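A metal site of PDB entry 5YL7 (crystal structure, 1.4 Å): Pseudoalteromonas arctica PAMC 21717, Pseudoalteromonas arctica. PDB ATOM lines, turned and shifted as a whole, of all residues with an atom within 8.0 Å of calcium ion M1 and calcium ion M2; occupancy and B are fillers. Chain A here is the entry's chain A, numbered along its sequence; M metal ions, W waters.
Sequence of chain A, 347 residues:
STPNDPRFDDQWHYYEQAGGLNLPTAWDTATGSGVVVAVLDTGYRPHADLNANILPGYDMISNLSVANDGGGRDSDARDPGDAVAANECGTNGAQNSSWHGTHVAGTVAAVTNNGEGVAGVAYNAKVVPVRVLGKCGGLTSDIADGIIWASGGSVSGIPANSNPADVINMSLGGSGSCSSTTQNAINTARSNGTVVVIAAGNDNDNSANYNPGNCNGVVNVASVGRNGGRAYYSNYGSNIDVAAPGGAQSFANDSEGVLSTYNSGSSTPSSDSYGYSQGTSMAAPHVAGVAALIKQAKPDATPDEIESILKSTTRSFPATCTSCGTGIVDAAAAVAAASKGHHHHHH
OD2 of Asp 69 lies close to NH1 of Arg 131. OD1 of Asp 59 lies within salt-bridge range of NH1 of Arg 131 (3.8 Å). The side-chain carboxylate (OD1) of Asp 59 sits at hydrogen-bond distance from the backbone NH (N) of Ile 61, 3.1 Å away. The side-chain carboxylate (OD1) of Asp 76 sits at hydrogen-bond distance from the backbone NH (N) of Arg 78, 3.0 Å away.
Four residues have an atom within 4 Å of calcium ion M1: Asp 69, Gly 71, Gly 72 and Asp 74.
Within 4 Å of calcium ion M2: Asp 59, Asp 69, Asp 74 and Asp 76.
Calcium ion M1 is bound by O of Gly 72 (2.3 Å), water W3 (2.3 Å), water W4 (2.3 Å), OD2 of Asp 74 (2.4 Å), O of Gly 71 (2.4 Å), OD1 of Asp 69 (2.5 Å) and OD2 of Asp 69 (2.5 Å).
Calcium ion M2 is bound by OD2 of Asp 69 (2.3 Å), water W1 (2.4 Å), water W2 (2.4 Å), OD2 of Asp 59 (2.4 Å), O of Asp 76 (2.4 Å), OD1 of Asp 74 (2.5 Å) and OD2 of Asp 74 (2.5 Å). Calcium ion M2 has seven donor atoms within binding distance.
Water W4 bridges the backbone carbonyl oxygen of Ile 61 and the side-chain carboxylate of Asp 59.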
ATOM      1  N   TYR A  58     -35.060 -15.085  -9.632  1.00  0.00           N
ATOM      2  CA  TYR A  58     -33.990 -15.936  -9.137  1.00  0.00           C
ATOM      3  C   TYR A  58     -33.458 -16.816 -10.226  1.00  0.00           C
ATOM      4  O   TYR A  58     -34.203 -17.146 -11.189  1.00  0.00           O
ATOM      5  CB  TYR A  58     -34.474 -16.849  -7.975  1.00  0.00           C
ATOM      6  CG  TYR A  58     -33.337 -17.089  -6.954  1.00  0.00           C
ATOM      7  CD1 TYR A  58     -33.040 -16.141  -6.034  1.00  0.00           C
ATOM      8  CD2 TYR A  58     -32.480 -18.186  -7.023  1.00  0.00           C
ATOM      9  CE1 TYR A  58     -31.971 -16.224  -5.184  1.00  0.00           C
ATOM     10  CE2 TYR A  58     -31.384 -18.265  -6.106  1.00  0.00           C
ATOM     11  CZ  TYR A  58     -31.217 -17.209  -5.293  1.00  0.00           C
ATOM     12  OH  TYR A  58     -30.080 -17.322  -4.412  1.00  0.00           O
ATOM     13  N   ASP A  59     -32.188 -17.171 -10.177  1.00  0.00           N
ATOM     14  CA  ASP A  59     -31.493 -17.989 -11.122  1.00  0.00           C
ATOM     15  C   ASP A  59     -31.179 -19.307 -10.477  1.00  0.00           C
ATOM     16  O   ASP A  59     -30.344 -19.412  -9.555  1.00  0.00           O
ATOM     17  CB  ASP A  59     -30.236 -17.243 -11.609  1.00  0.00           C
ATOM     18  CG  ASP A  59     -29.520 -17.956 -12.682  1.00  0.00           C
ATOM     19  OD1 ASP A  59     -29.575 -19.161 -12.892  1.00  0.00           O
ATOM     20  OD2 ASP A  59     -28.709 -17.219 -13.396  1.00  0.00           O
ATOM     21  N   MET A  60     -31.899 -20.360 -10.891  1.00  0.00           N
ATOM     22  CA  MET A  60     -31.812 -21.673 -10.344  1.00  0.00           C
ATOM     23  C   MET A  60     -30.810 -22.527 -10.942  1.00  0.00           C
ATOM     24  O   MET A  60     -30.655 -23.744 -10.585  1.00  0.00           O
ATOM     25  CB  MET A  60     -33.156 -22.382 -10.488  1.00  0.00           C
ATOM     26  CG  MET A  60     -34.271 -21.744  -9.753  1.00  0.00           C
ATOM     27  SD  MET A  60     -33.905 -21.943  -7.880  1.00  0.00           S
ATOM     28  CE  MET A  60     -35.344 -20.974  -7.288  1.00  0.00           C
ATOM     29  N   ILE A  61     -30.045 -22.086 -11.935  1.00  0.00           N
ATOM     30  CA  ILE A  61     -29.121 -22.953 -12.653  1.00  0.00           C
ATOM     31  C   ILE A  61     -27.878 -23.282 -11.785  1.00  0.00           C
ATOM     32  O   ILE A  61     -27.130 -22.398 -11.365  1.00  0.00           O
ATOM     33  CB  ILE A  61     -28.690 -22.409 -14.002  1.00  0.00           C
ATOM     34  CG1 ILE A  61     -29.875 -22.103 -14.861  1.00  0.00           C
ATOM     35  CG2 ILE A  61     -27.753 -23.430 -14.653  1.00  0.00           C
ATOM     36  CD1 ILE A  61     -29.501 -21.396 -16.132  1.00  0.00           C
ATOM     37  N   SER A  62     -27.776 -24.576 -11.459  1.00  0.00           N
ATOM     38  CA  SER A  62     -26.676 -25.047 -10.544  1.00  0.00           C
ATOM     39  C   SER A  62     -25.395 -25.368 -11.301  1.00  0.00           C
ATOM     40  O   SER A  62     -24.290 -25.143 -10.727  1.00  0.00           O
ATOM     41  CB  SER A  62     -27.180 -26.311  -9.775  1.00  0.00           C
ATOM     42  OG  SER A  62     -28.370 -26.135  -9.118  1.00  0.00           O
ATOM     43  N   ASN A  63     -25.451 -25.840 -12.517  1.00  0.00           N
ATOM     44  CA  ASN A  63     -24.245 -26.216 -13.275  1.00  0.00           C
ATOM     45  C   ASN A  63     -23.576 -24.993 -13.860  1.00  0.00           C
ATOM     46  O   ASN A  63     -24.261 -24.219 -14.593  1.00  0.00           O
ATOM     47  CB  ASN A  63     -24.670 -27.241 -14.302  1.00  0.00           C
ATOM     48  CG  ASN A  63     -23.563 -27.665 -15.251  1.00  0.00           C
ATOM     49  OD1 ASN A  63     -22.905 -26.890 -15.920  1.00  0.00           O
ATOM     50  ND2 ASN A  63     -23.474 -28.960 -15.441  1.00  0.00           N
ATOM     51  N   LEU A  64     -22.339 -24.716 -13.531  1.00  0.00           N
ATOM     52  CA  LEU A  64     -21.700 -23.496 -13.917  1.00  0.00           C
ATOM     53  C   LEU A  64     -21.576 -23.390 -15.420  1.00  0.00           C
ATOM     54  O   LEU A  64     -21.661 -22.261 -15.926  1.00  0.00           O
ATOM     55  CB  LEU A  64     -20.276 -23.408 -13.251  1.00  0.00           C
ATOM     56  CG  LEU A  64     -20.386 -22.580 -11.936  1.00  0.00           C
ATOM     57  CD1 LEU A  64     -21.157 -23.267 -10.828  1.00  0.00           C
ATOM     58  CD2 LEU A  64     -18.999 -22.190 -11.439  1.00  0.00           C
ATOM     59  N   VAL A  66     -23.619 -24.529 -17.742  1.00  0.00           N
ATOM     60  CA  VAL A  66     -24.937 -24.218 -18.258  1.00  0.00           C
ATOM     61  C   VAL A  66     -25.223 -22.759 -17.874  1.00  0.00           C
ATOM     62  O   VAL A  66     -25.743 -21.958 -18.703  1.00  0.00           O
ATOM     63  CB  VAL A  66     -25.995 -25.137 -17.688  1.00  0.00           C
ATOM     64  CG1 VAL A  66     -27.358 -24.758 -18.144  1.00  0.00           C
ATOM     65  CG2 VAL A  66     -25.716 -26.600 -18.126  1.00  0.00           C
ATOM     66  N   ALA A  67     -24.929 -22.367 -16.659  1.00  0.00           N
ATOM     67  CA  ALA A  67     -25.300 -21.073 -16.136  1.00  0.00           C
ATOM     68  C   ALA A  67     -24.630 -19.943 -16.917  1.00  0.00           C
ATOM     69  O   ALA A  67     -25.246 -18.892 -17.151  1.00  0.00           O
ATOM     70  CB  ALA A  67     -24.884 -20.932 -14.698  1.00  0.00           C
ATOM     71  N   ASN A  68     -23.346 -20.050 -17.279  1.00  0.00           N
ATOM     72  CA  ASN A  68     -22.666 -19.112 -18.120  1.00  0.00           C
ATOM     73  C   ASN A  68     -22.697 -17.756 -17.489  1.00  0.00           C
ATOM     74  O   ASN A  68     -22.732 -16.762 -18.237  1.00  0.00           O
ATOM     75  CB  ASN A  68     -23.276 -19.076 -19.538  1.00  0.00           C
ATOM     76  CG  ASN A  68     -22.472 -18.276 -20.533  1.00  0.00           C
ATOM     77  OD1 ASN A  68     -21.226 -18.274 -20.470  1.00  0.00           O
ATOM     78  ND2 ASN A  68     -23.121 -17.551 -21.418  1.00  0.00           N
ATOM     79  N   ASP A  69     -22.596 -17.628 -16.179  1.00  0.00           N
ATOM     80  CA  ASP A  69     -22.624 -16.351 -15.475  1.00  0.00           C
ATOM     81  C   ASP A  69     -21.645 -16.288 -14.309  1.00  0.00           C
ATOM     82  O   ASP A  69     -21.688 -15.355 -13.554  1.00  0.00           O
ATOM     83  CB  ASP A  69     -24.057 -16.041 -15.008  1.00  0.00           C
ATOM     84  CG  ASP A  69     -24.549 -16.959 -13.940  1.00  0.00           C
ATOM     85  OD1 ASP A  69     -23.788 -17.889 -13.538  1.00  0.00           O
ATOM     86  OD2 ASP A  69     -25.685 -16.706 -13.387  1.00  0.00           O
ATOM     87  N   GLY A  70     -20.780 -17.275 -14.210  1.00  0.00           N
ATOM     88  CA  GLY A  70     -19.678 -17.210 -13.234  1.00  0.00           C
ATOM     89  C   GLY A  70     -19.953 -17.976 -11.981  1.00  0.00           C
ATOM     90  O   GLY A  70     -19.004 -18.119 -11.132  1.00  0.00           O
ATOM     91  N   GLY A  71     -21.110 -18.596 -11.737  1.00  0.00           N
ATOM     92  CA  GLY A  71     -21.391 -19.308 -10.530  1.00  0.00           C
ATOM     93  C   GLY A  71     -22.695 -20.017 -10.604  1.00  0.00           C
ATOM     94  O   GLY A  71     -23.440 -19.999 -11.620  1.00  0.00           O
ATOM     95  N   GLY A  72     -22.976 -20.718  -9.550  1.00  0.00           N
ATOM     96  CA  GLY A  72     -24.240 -21.460  -9.352  1.00  0.00           C
ATOM     97  C   GLY A  72     -25.406 -20.623  -9.078  1.00  0.00           C
ATOM     98  O   GLY A  72     -25.532 -19.472  -9.569  1.00  0.00           O
ATOM     99  N   ARG A  73     -26.328 -21.088  -8.284  1.00  0.00           N
ATOM    100  CA  ARG A  73     -27.575 -20.381  -8.042  1.00  0.00           C
ATOM    101  C   ARG A  73     -27.316 -18.996  -7.574  1.00  0.00           C
ATOM    102  O   ARG A  73     -26.458 -18.750  -6.710  1.00  0.00           O
ATOM    103  CB  ARG A  73     -28.559 -21.219  -7.180  1.00  0.00           C
ATOM    104  CG  ARG A  73     -28.958 -22.515  -7.853  1.00  0.00           C
ATOM    105  CD  ARG A  73     -30.049 -23.207  -6.997  1.00  0.00           C
ATOM    106  NE  ARG A  73     -30.597 -24.323  -7.731  1.00  0.00           N
ATOM    107  CZ  ARG A  73     -31.470 -25.204  -7.221  1.00  0.00           C
ATOM    108  NH1 ARG A  73     -31.853 -25.082  -5.961  1.00  0.00           N
ATOM    109  NH2 ARG A  73     -31.952 -26.074  -8.027  1.00  0.00           N
ATOM    110  N   ASP A  74     -28.129 -18.050  -7.995  1.00  0.00           N
ATOM    111  CA  ASP A  74     -27.908 -16.664  -7.647  1.00  0.00           C
ATOM    112  C   ASP A  74     -29.122 -15.825  -7.856  1.00  0.00           C
ATOM    113  O   ASP A  74     -30.067 -16.259  -8.564  1.00  0.00           O
ATOM    114  CB  ASP A  74     -26.754 -16.063  -8.449  1.00  0.00           C
ATOM    115  CG  ASP A  74     -27.059 -15.906  -9.933  1.00  0.00           C
ATOM    116  OD1 ASP A  74     -27.598 -14.811 -10.280  1.00  0.00           O
ATOM    117  OD2 ASP A  74     -26.810 -16.776 -10.751  1.00  0.00           O
ATOM    118  N   SER A  75     -29.199 -14.614  -7.354  1.00  0.00           N
ATOM    119  CA  SER A  75     -30.391 -13.807  -7.397  1.00  0.00           C
ATOM    120  C   SER A  75     -30.618 -13.046  -8.724  1.00  0.00           C
ATOM    121  O   SER A  75     -31.673 -12.449  -8.814  1.00  0.00           O
ATOM    122  CB  SER A  75     -30.527 -12.856  -6.207  1.00  0.00           C
ATOM    123  OG  SER A  75     -29.526 -11.897  -6.352  1.00  0.00           O
ATOM    124  N   ASP A  76     -29.681 -13.107  -9.657  1.00  0.00           N
ATOM    125  CA  ASP A  76     -29.837 -12.304 -10.903  1.00  0.00           C
ATOM    126  C   ASP A  76     -30.253 -13.265 -12.013  1.00  0.00           C
ATOM    127  O   ASP A  76     -29.488 -14.062 -12.520  1.00  0.00           O
ATOM    128  CB  ASP A  76     -28.505 -11.652 -11.199  1.00  0.00           C
ATOM    129  CG  ASP A  76     -28.570 -10.760 -12.355  1.00  0.00           C
ATOM    130  OD1 ASP A  76     -29.577 -10.697 -13.081  1.00  0.00           O
ATOM    131  OD2 ASP A  76     -27.629  -9.930 -12.568  1.00  0.00           O
ATOM    132  N   ALA A  77     -31.519 -13.132 -12.425  1.00  0.00           N
ATOM    133  CA  ALA A  77     -32.131 -13.987 -13.441  1.00  0.00           C
ATOM    134  C   ALA A  77     -31.956 -13.443 -14.812  1.00  0.00           C
ATOM    135  O   ALA A  77     -32.613 -13.861 -15.778  1.00  0.00           O
ATOM    136  CB  ALA A  77     -33.618 -14.162 -13.123  1.00  0.00           C
ATOM    137  N   ARG A  78     -31.068 -12.436 -15.038  1.00  0.00           N
ATOM    138  CA  ARG A  78     -30.785 -12.026 -16.381  1.00  0.00           C
ATOM    139  C   ARG A  78     -30.169 -13.109 -17.209  1.00  0.00           C
ATOM    140  O   ARG A  78     -29.464 -13.990 -16.710  1.00  0.00           O
ATOM    141  CB  ARG A  78     -29.948 -10.746 -16.401  1.00  0.00           C
ATOM    142  CG  ARG A  78     -30.731  -9.543 -16.005  1.00  0.00           C
ATOM    143  CD  ARG A  78     -29.926  -8.269 -15.940  1.00  0.00           C
ATOM    144  NE  ARG A  78     -30.720  -7.155 -15.485  1.00  0.00           N
ATOM    145  CZ  ARG A  78     -30.421  -5.844 -15.654  1.00  0.00           C
ATOM    146  NH1 ARG A  78     -29.368  -5.497 -16.321  1.00  0.00           N
ATOM    147  NH2 ARG A  78     -31.237  -4.951 -15.167  1.00  0.00           N
ATOM    148  N   ASP A  79     -30.424 -13.073 -18.532  1.00  0.00           N
ATOM    149  CA  ASP A  79     -29.926 -14.053 -19.454  1.00  0.00           C
ATOM    150  C   ASP A  79     -28.569 -13.607 -19.964  1.00  0.00           C
ATOM    151  O   ASP A  79     -28.507 -12.591 -20.679  1.00  0.00           O
ATOM    152  CB  ASP A  79     -30.906 -14.175 -20.618  1.00  0.00           C
ATOM    153  CG  ASP A  79     -30.653 -15.275 -21.564  1.00  0.00           C
ATOM    154  OD1 ASP A  79     -29.565 -15.911 -21.512  1.00  0.00           O
ATOM    155  OD2 ASP A  79     -31.524 -15.505 -22.459  1.00  0.00           O
ATOM    156  N   PRO A  80     -27.495 -14.342 -19.691  1.00  0.00           N
ATOM    157  CA  PRO A  80     -26.160 -13.980 -20.246  1.00  0.00           C
ATOM    158  C   PRO A  80     -26.014 -14.335 -21.664  1.00  0.00           C
ATOM    159  O   PRO A  80     -24.970 -13.982 -22.270  1.00  0.00           O
ATOM    160  CB  PRO A  80     -25.233 -14.750 -19.360  1.00  0.00           C
ATOM    161  CG  PRO A  80     -25.984 -16.059 -19.028  1.00  0.00           C
ATOM    162  CD  PRO A  80     -27.424 -15.558 -18.900  1.00  0.00           C
ATOM    163  N   ARG A 131     -34.856 -18.039 -13.841  1.00  0.00           N
ATOM    164  CA  ARG A 131     -33.932 -18.525 -14.814  1.00  0.00           C
ATOM    165  C   ARG A 131     -33.614 -19.983 -14.534  1.00  0.00           C
ATOM    166  O   ARG A 131     -33.001 -20.287 -13.506  1.00  0.00           O
ATOM    167  CB  ARG A 131     -32.665 -17.654 -14.956  1.00  0.00           C
ATOM    168  CG  ARG A 131     -31.686 -18.200 -15.914  1.00  0.00           C
ATOM    169  CD  ARG A 131     -30.638 -17.158 -16.276  1.00  0.00           C
ATOM    170  NE  ARG A 131     -29.770 -17.712 -17.290  1.00  0.00           N
ATOM    171  CZ  ARG A 131     -28.512 -18.155 -17.181  1.00  0.00           C
ATOM    172  NH1 ARG A 131     -27.872 -18.048 -16.050  1.00  0.00           N
ATOM    173  NH2 ARG A 131     -27.921 -18.721 -18.202  1.00  0.00           N
HETATM  174 CA    CA M   1     -25.220 -18.342 -11.565  1.00  0.00          CA
HETATM  175 CA    CA M   2     -27.454 -15.327 -12.735  1.00  0.00          CA
HETATM  176  O   HOH W   1     -27.480 -14.363 -14.881  1.00  0.00           O
HETATM  177  O   HOH W   2     -25.727 -13.752 -12.412  1.00  0.00           O
HETATM  178  O   HOH W   3     -23.671 -17.062 -10.358  1.00  0.00           O
HETATM  179  O   HOH W   4     -26.896 -19.809 -12.306  1.00  0.00           O
